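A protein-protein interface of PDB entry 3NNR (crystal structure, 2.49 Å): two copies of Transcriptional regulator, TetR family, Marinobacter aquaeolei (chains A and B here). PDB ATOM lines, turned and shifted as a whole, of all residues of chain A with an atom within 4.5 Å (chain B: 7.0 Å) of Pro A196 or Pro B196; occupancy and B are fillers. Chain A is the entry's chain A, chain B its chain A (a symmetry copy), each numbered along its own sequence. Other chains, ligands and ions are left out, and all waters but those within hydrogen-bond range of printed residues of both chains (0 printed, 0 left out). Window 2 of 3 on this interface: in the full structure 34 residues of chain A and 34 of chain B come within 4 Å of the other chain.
SD of Met B151 lies close to OH of Tyr B197, 3.8 Å away. The backbone NH (N) of Gln B141 is in hydrogen-bond range of the backbone carbonyl oxygen (O) of Tyr B197, 2.8 Å away.
Among the printed residues, pairs that only touch across the chains: Thr A192 with Leu B147 (3.8 Å), Leu A193 with Leu B193 (3.4 Å), Pro A196 with Pro B196 (3.7 Å), Pro A196 with Tyr B197 (3.4 Å) and Tyr A197 with Pro B196 (3.4 Å).
Pro A196 touches just these residues of chain B: Pro B196 and Tyr B197. Pro B196 touches just these residues of chain A: Pro A196 (3.7 Å) and Tyr A197 (3.4 Å). Of the printed residues of chain A, Leu B147 touches Thr A192. Of the printed residues of chain A, Tyr B197 touches Pro A196 (3.4 Å). Of the printed residues of chain B, Thr A192 touches Leu B147. Of the printed residues of chain A, Leu B193 touches Leu A193 (3.4 Å). Thr B192 touches none of the printed residues of chain A. The nearest printed residue of chain B that does not touch Thr A192 is Met B151 (4.2 Å).
Hydrophobic or aromatic side chains of chain A within 4 Å of the printed part of chain B: Leu A193, Pro A196 and Tyr A197. Of the 14 printed residues of chain B, 4 touch a printed residue of chain A.
Leu A193 touches its own counterpart, Leu B193. Pro A196 touches its own counterpart, Pro B196. Pro A196 touches Tyr B197, and with the chains exchanged Tyr A197 touches Pro B196.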
ATOM      1  N   THR A 192      -0.131 -22.282  -8.011  1.00  0.00           N
ATOM      2  CA  THR A 192      -1.116 -23.303  -8.354  1.00  0.00           C
ATOM      3  C   THR A 192      -0.816 -23.900  -9.732  1.00  0.00           C
ATOM      4  O   THR A 192      -1.096 -25.074  -9.948  1.00  0.00           O
ATOM      5  CB  THR A 192      -2.544 -22.736  -8.328  1.00  0.00           C
ATOM      6  OG1 THR A 192      -2.813 -22.245  -7.010  1.00  0.00           O
ATOM      7  CG2 THR A 192      -3.574 -23.781  -8.695  1.00  0.00           C
ATOM      8  N   LEU A 193      -0.241 -23.109 -10.643  1.00  0.00           N
ATOM      9  CA  LEU A 193       0.138 -23.617 -11.972  1.00  0.00           C
ATOM     10  C   LEU A 193       1.186 -24.729 -11.889  1.00  0.00           C
ATOM     11  O   LEU A 193       1.106 -25.671 -12.662  1.00  0.00           O
ATOM     12  CB  LEU A 193       0.669 -22.513 -12.901  1.00  0.00           C
ATOM     13  CG  LEU A 193      -0.260 -21.360 -13.217  1.00  0.00           C
ATOM     14  CD1 LEU A 193       0.506 -20.271 -13.973  1.00  0.00           C
ATOM     15  CD2 LEU A 193      -1.471 -21.868 -14.004  1.00  0.00           C
ATOM     16  N   GLU A 194       2.121 -24.630 -10.950  1.00  0.00           N
ATOM     17  CA  GLU A 194       3.203 -25.623 -10.813  1.00  0.00           C
ATOM     18  C   GLU A 194       3.004 -26.667  -9.709  1.00  0.00           C
ATOM     19  O   GLU A 194       3.898 -27.475  -9.524  1.00  0.00           O
ATOM     20  CB  GLU A 194       4.566 -24.919 -10.686  1.00  0.00           C
ATOM     21  CG  GLU A 194       4.899 -23.936 -11.861  1.00  0.00           C
ATOM     22  CD  GLU A 194       5.002 -24.588 -13.268  1.00  0.00           C
ATOM     23  OE1 GLU A 194       5.669 -25.653 -13.415  1.00  0.00           O
ATOM     24  OE2 GLU A 194       4.440 -24.000 -14.234  1.00  0.00           O
ATOM     25  N   VAL A 195       1.848 -26.680  -9.024  1.00  0.00           N
ATOM     26  CA  VAL A 195       1.509 -27.705  -8.002  1.00  0.00           C
ATOM     27  C   VAL A 195       1.696 -29.180  -8.439  1.00  0.00           C
ATOM     28  O   VAL A 195       2.383 -29.922  -7.737  1.00  0.00           O
ATOM     29  CB  VAL A 195       0.045 -27.530  -7.426  1.00  0.00           C
ATOM     30  CG1 VAL A 195      -0.493 -28.842  -6.735  1.00  0.00           C
ATOM     31  CG2 VAL A 195      -0.009 -26.344  -6.466  1.00  0.00           C
ATOM     32  N   PRO A 196       1.082 -29.612  -9.564  1.00  0.00           N
ATOM     33  CA  PRO A 196       1.245 -31.022  -9.975  1.00  0.00           C
ATOM     34  C   PRO A 196       2.630 -31.417 -10.527  1.00  0.00           C
ATOM     35  O   PRO A 196       2.906 -32.619 -10.602  1.00  0.00           O
ATOM     36  CB  PRO A 196       0.172 -31.198 -11.040  1.00  0.00           C
ATOM     37  CG  PRO A 196       0.068 -29.862 -11.650  1.00  0.00           C
ATOM     38  CD  PRO A 196       0.289 -28.865 -10.554  1.00  0.00           C
ATOM     39  N   TYR A 197       3.462 -30.441 -10.917  1.00  0.00           N
ATOM     40  CA  TYR A 197       4.829 -30.709 -11.404  1.00  0.00           C
ATOM     41  C   TYR A 197       5.918 -30.709 -10.301  1.00  0.00           C
ATOM     42  O   TYR A 197       7.110 -30.916 -10.610  1.00  0.00           O
ATOM     43  CB  TYR A 197       5.226 -29.723 -12.509  1.00  0.00           C
ATOM     44  CG  TYR A 197       4.282 -29.700 -13.691  1.00  0.00           C
ATOM     45  CD1 TYR A 197       4.151 -30.824 -14.536  1.00  0.00           C
ATOM     46  CD2 TYR A 197       3.529 -28.547 -13.992  1.00  0.00           C
ATOM     47  CE1 TYR A 197       3.268 -30.810 -15.647  1.00  0.00           C
ATOM     48  CE2 TYR A 197       2.651 -28.522 -15.096  1.00  0.00           C
ATOM     49  CZ  TYR A 197       2.532 -29.650 -15.922  1.00  0.00           C
ATOM     50  OH  TYR A 197       1.679 -29.602 -17.002  1.00  0.00           O
ATOM     51  N   LEU A 198       5.536 -30.490  -9.038  1.00  0.00           N
ATOM     52  CA  LEU A 198       6.505 -30.493  -7.946  1.00  0.00           C
ATOM     53  C   LEU A 198       7.075 -31.905  -7.743  1.00  0.00           C
ATOM     54  O   LEU A 198       6.322 -32.887  -7.768  1.00  0.00           O
ATOM     55  CB  LEU A 198       5.880 -29.983  -6.639  1.00  0.00           C
ATOM     56  CG  LEU A 198       5.382 -28.528  -6.608  1.00  0.00           C
ATOM     57  CD1 LEU A 198       4.668 -28.237  -5.326  1.00  0.00           C
ATOM     58  CD2 LEU A 198       6.504 -27.522  -6.796  1.00  0.00           C
ATOM     59  N   GLN B 141      -8.818 -36.039 -13.323  1.00  0.00           N
ATOM     60  CA  GLN B 141      -8.727 -36.641 -11.988  1.00  0.00           C
ATOM     61  C   GLN B 141      -9.481 -35.728 -11.012  1.00  0.00           C
ATOM     62  O   GLN B 141      -9.365 -34.511 -11.120  1.00  0.00           O
ATOM     63  CB  GLN B 141      -7.265 -36.841 -11.596  1.00  0.00           C
ATOM     64  CG  GLN B 141      -6.598 -37.914 -12.474  1.00  0.00           C
ATOM     65  CD  GLN B 141      -5.083 -38.035 -12.321  1.00  0.00           C
ATOM     66  OE1 GLN B 141      -4.424 -37.248 -11.624  1.00  0.00           O
ATOM     67  NE2 GLN B 141      -4.522 -39.033 -12.994  1.00  0.00           N
ATOM     68  N   GLN B 143     -10.340 -33.451  -7.957  1.00  0.00           N
ATOM     69  CA  GLN B 143      -9.449 -32.642  -7.113  1.00  0.00           C
ATOM     70  C   GLN B 143     -10.133 -32.048  -5.868  1.00  0.00           C
ATOM     71  O   GLN B 143     -11.347 -31.833  -5.896  1.00  0.00           O
ATOM     72  CB  GLN B 143      -8.790 -31.544  -7.972  1.00  0.00           C
ATOM     73  CG  GLN B 143      -7.817 -32.064  -9.067  1.00  0.00           C
ATOM     74  CD  GLN B 143      -6.632 -32.923  -8.518  1.00  0.00           C
ATOM     75  OE1 GLN B 143      -6.152 -32.731  -7.388  1.00  0.00           O
ATOM     76  NE2 GLN B 143      -6.166 -33.870  -9.336  1.00  0.00           N
ATOM     77  N   LEU B 147      -8.038 -26.705  -4.316  1.00  0.00           N
ATOM     78  CA  LEU B 147      -7.230 -26.748  -5.550  1.00  0.00           C
ATOM     79  C   LEU B 147      -8.082 -26.563  -6.827  1.00  0.00           C
ATOM     80  O   LEU B 147      -7.586 -26.040  -7.827  1.00  0.00           O
ATOM     81  CB  LEU B 147      -6.394 -28.030  -5.598  1.00  0.00           C
ATOM     82  CG  LEU B 147      -5.493 -28.340  -6.803  1.00  0.00           C
ATOM     83  CD1 LEU B 147      -4.734 -27.115  -7.307  1.00  0.00           C
ATOM     84  CD2 LEU B 147      -4.502 -29.504  -6.467  1.00  0.00           C
ATOM     85  N   MET B 151      -7.795 -23.548  -9.439  1.00  0.00           N
ATOM     86  CA  MET B 151      -7.690 -23.844 -10.874  1.00  0.00           C
ATOM     87  C   MET B 151      -8.738 -23.156 -11.727  1.00  0.00           C
ATOM     88  O   MET B 151      -8.432 -22.784 -12.856  1.00  0.00           O
ATOM     89  CB  MET B 151      -7.710 -25.343 -11.141  1.00  0.00           C
ATOM     90  CG  MET B 151      -6.353 -25.946 -11.009  1.00  0.00           C
ATOM     91  SD  MET B 151      -6.482 -27.797 -10.664  1.00  0.00           S
ATOM     92  CE  MET B 151      -8.112 -28.330 -11.704  1.00  0.00           C
ATOM     93  N   LEU B 191      -6.432 -25.360 -22.027  1.00  0.00           N
ATOM     94  CA  LEU B 191      -6.278 -26.815 -21.946  1.00  0.00           C
ATOM     95  C   LEU B 191      -4.918 -27.218 -21.355  1.00  0.00           C
ATOM     96  O   LEU B 191      -4.798 -28.283 -20.750  1.00  0.00           O
ATOM     97  CB  LEU B 191      -6.582 -27.480 -23.297  1.00  0.00           C
ATOM     98  CG  LEU B 191      -8.039 -27.334 -23.782  1.00  0.00           C
ATOM     99  CD1 LEU B 191      -8.193 -27.832 -25.190  1.00  0.00           C
ATOM    100  CD2 LEU B 191      -9.039 -28.066 -22.893  1.00  0.00           C
ATOM    101  N   THR B 192      -3.919 -26.350 -21.503  1.00  0.00           N
ATOM    102  CA  THR B 192      -2.614 -26.549 -20.882  1.00  0.00           C
ATOM    103  C   THR B 192      -2.744 -26.598 -19.357  1.00  0.00           C
ATOM    104  O   THR B 192      -1.971 -27.300 -18.714  1.00  0.00           O
ATOM    105  CB  THR B 192      -1.625 -25.446 -21.289  1.00  0.00           C
ATOM    106  OG1 THR B 192      -1.478 -25.470 -22.713  1.00  0.00           O
ATOM    107  CG2 THR B 192      -0.271 -25.633 -20.641  1.00  0.00           C
ATOM    108  N   LEU B 193      -3.716 -25.877 -18.790  1.00  0.00           N
ATOM    109  CA  LEU B 193      -3.952 -25.913 -17.338  1.00  0.00           C
ATOM    110  C   LEU B 193      -4.341 -27.311 -16.849  1.00  0.00           C
ATOM    111  O   LEU B 193      -3.912 -27.698 -15.774  1.00  0.00           O
ATOM    112  CB  LEU B 193      -5.035 -24.919 -16.887  1.00  0.00           C
ATOM    113  CG  LEU B 193      -4.795 -23.451 -17.167  1.00  0.00           C
ATOM    114  CD1 LEU B 193      -6.057 -22.648 -16.842  1.00  0.00           C
ATOM    115  CD2 LEU B 193      -3.578 -22.961 -16.376  1.00  0.00           C
ATOM    116  N   GLU B 194      -5.107 -28.053 -17.642  1.00  0.00           N
ATOM    117  CA  GLU B 194      -5.576 -29.394 -17.247  1.00  0.00           C
ATOM    118  C   GLU B 194      -4.794 -30.569 -17.846  1.00  0.00           C
ATOM    119  O   GLU B 194      -5.179 -31.697 -17.590  1.00  0.00           O
ATOM    120  CB  GLU B 194      -7.087 -29.533 -17.503  1.00  0.00           C
ATOM    121  CG  GLU B 194      -7.965 -28.441 -16.801  1.00  0.00           C
ATOM    122  CD  GLU B 194      -7.900 -28.429 -15.248  1.00  0.00           C
ATOM    123  OE1 GLU B 194      -8.001 -29.517 -14.611  1.00  0.00           O
ATOM    124  OE2 GLU B 194      -7.787 -27.312 -14.670  1.00  0.00           O
ATOM    125  N   VAL B 195      -3.701 -30.315 -18.586  1.00  0.00           N
ATOM    126  CA  VAL B 195      -2.814 -31.376 -19.133  1.00  0.00           C
ATOM    127  C   VAL B 195      -2.333 -32.442 -18.117  1.00  0.00           C
ATOM    128  O   VAL B 195      -2.513 -33.631 -18.379  1.00  0.00           O
ATOM    129  CB  VAL B 195      -1.551 -30.786 -19.883  1.00  0.00           C
ATOM    130  CG1 VAL B 195      -0.390 -31.844 -20.035  1.00  0.00           C
ATOM    131  CG2 VAL B 195      -1.958 -30.220 -21.242  1.00  0.00           C
ATOM    132  N   PRO B 196      -1.712 -32.036 -16.986  1.00  0.00           N
ATOM    133  CA  PRO B 196      -1.238 -33.052 -16.023  1.00  0.00           C
ATOM    134  C   PRO B 196      -2.326 -33.787 -15.214  1.00  0.00           C
ATOM    135  O   PRO B 196      -2.013 -34.828 -14.628  1.00  0.00           O
ATOM    136  CB  PRO B 196      -0.329 -32.254 -15.100  1.00  0.00           C
ATOM    137  CG  PRO B 196      -0.928 -30.910 -15.100  1.00  0.00           C
ATOM    138  CD  PRO B 196      -1.473 -30.677 -16.476  1.00  0.00           C
ATOM    139  N   TYR B 197      -3.556 -33.252 -15.168  1.00  0.00           N
ATOM    140  CA  TYR B 197      -4.680 -33.906 -14.471  1.00  0.00           C
ATOM    141  C   TYR B 197      -5.517 -34.864 -15.356  1.00  0.00           C
ATOM    142  O   TYR B 197      -6.498 -35.460 -14.864  1.00  0.00           O
ATOM    143  CB  TYR B 197      -5.608 -32.869 -13.826  1.00  0.00           C
ATOM    144  CG  TYR B 197      -4.918 -31.929 -12.864  1.00  0.00           C
ATOM    145  CD1 TYR B 197      -4.366 -32.406 -11.654  1.00  0.00           C
ATOM    146  CD2 TYR B 197      -4.830 -30.549 -13.139  1.00  0.00           C
ATOM    147  CE1 TYR B 197      -3.717 -31.530 -10.746  1.00  0.00           C
ATOM    148  CE2 TYR B 197      -4.190 -29.669 -12.242  1.00  0.00           C
ATOM    149  CZ  TYR B 197      -3.645 -30.163 -11.047  1.00  0.00           C
ATOM    150  OH  TYR B 197      -3.035 -29.286 -10.177  1.00  0.00           O
ATOM    151  N   LEU B 198      -5.150 -35.026 -16.631  1.00  0.00           N
ATOM    152  CA  LEU B 198      -5.882 -35.927 -17.518  1.00  0.00           C
ATOM    153  C   LEU B 198      -5.698 -37.384 -17.067  1.00  0.00           C
ATOM    154  O   LEU B 198      -4.580 -37.792 -16.726  1.00  0.00           O
ATOM    155  CB  LEU B 198      -5.433 -35.765 -18.978  1.00  0.00           C
ATOM    156  CG  LEU B 198      -5.675 -34.403 -19.650  1.00  0.00           C
ATOM    157  CD1 LEU B 198      -5.049 -34.361 -21.008  1.00  0.00           C
ATOM    158  CD2 LEU B 198      -7.151 -34.064 -19.769  1.00  0.00           C
ATOM    159  N   THR B 199      -6.808 -38.134 -17.034  1.00  0.00           N
ATOM    160  CA  THR B 199      -6.812 -39.569 -16.688  1.00  0.00           C
ATOM    161  C   THR B 199      -6.231 -40.405 -17.838  1.00  0.00           C
ATOM    162  O   THR B 199      -6.169 -39.924 -18.986  1.00  0.00           O
ATOM    163  CB  THR B 199      -8.245 -40.115 -16.442  1.00  0.00           C
ATOM    164  OG1 THR B 199      -9.043 -39.911 -17.618  1.00  0.00           O
ATOM    165  CG2 THR B 199      -8.911 -39.430 -15.261  1.00  0.00           C
ATOM    166  N   LEU B 207      -5.290 -34.245 -25.428  1.00  0.00           N
ATOM    167  CA  LEU B 207      -4.052 -33.690 -26.035  1.00  0.00           C
ATOM    168  C   LEU B 207      -4.198 -33.515 -27.553  1.00  0.00           C
ATOM    169  O   LEU B 207      -3.708 -32.528 -28.112  1.00  0.00           O
ATOM    170  CB  LEU B 207      -2.832 -34.567 -25.768  1.00  0.00           C
ATOM    171  CG  LEU B 207      -2.052 -34.442 -24.463  1.00  0.00           C
ATOM    172  CD1 LEU B 207      -2.939 -34.180 -23.276  1.00  0.00           C
ATOM    173  CD2 LEU B 207      -1.181 -35.695 -24.268  1.00  0.00           C
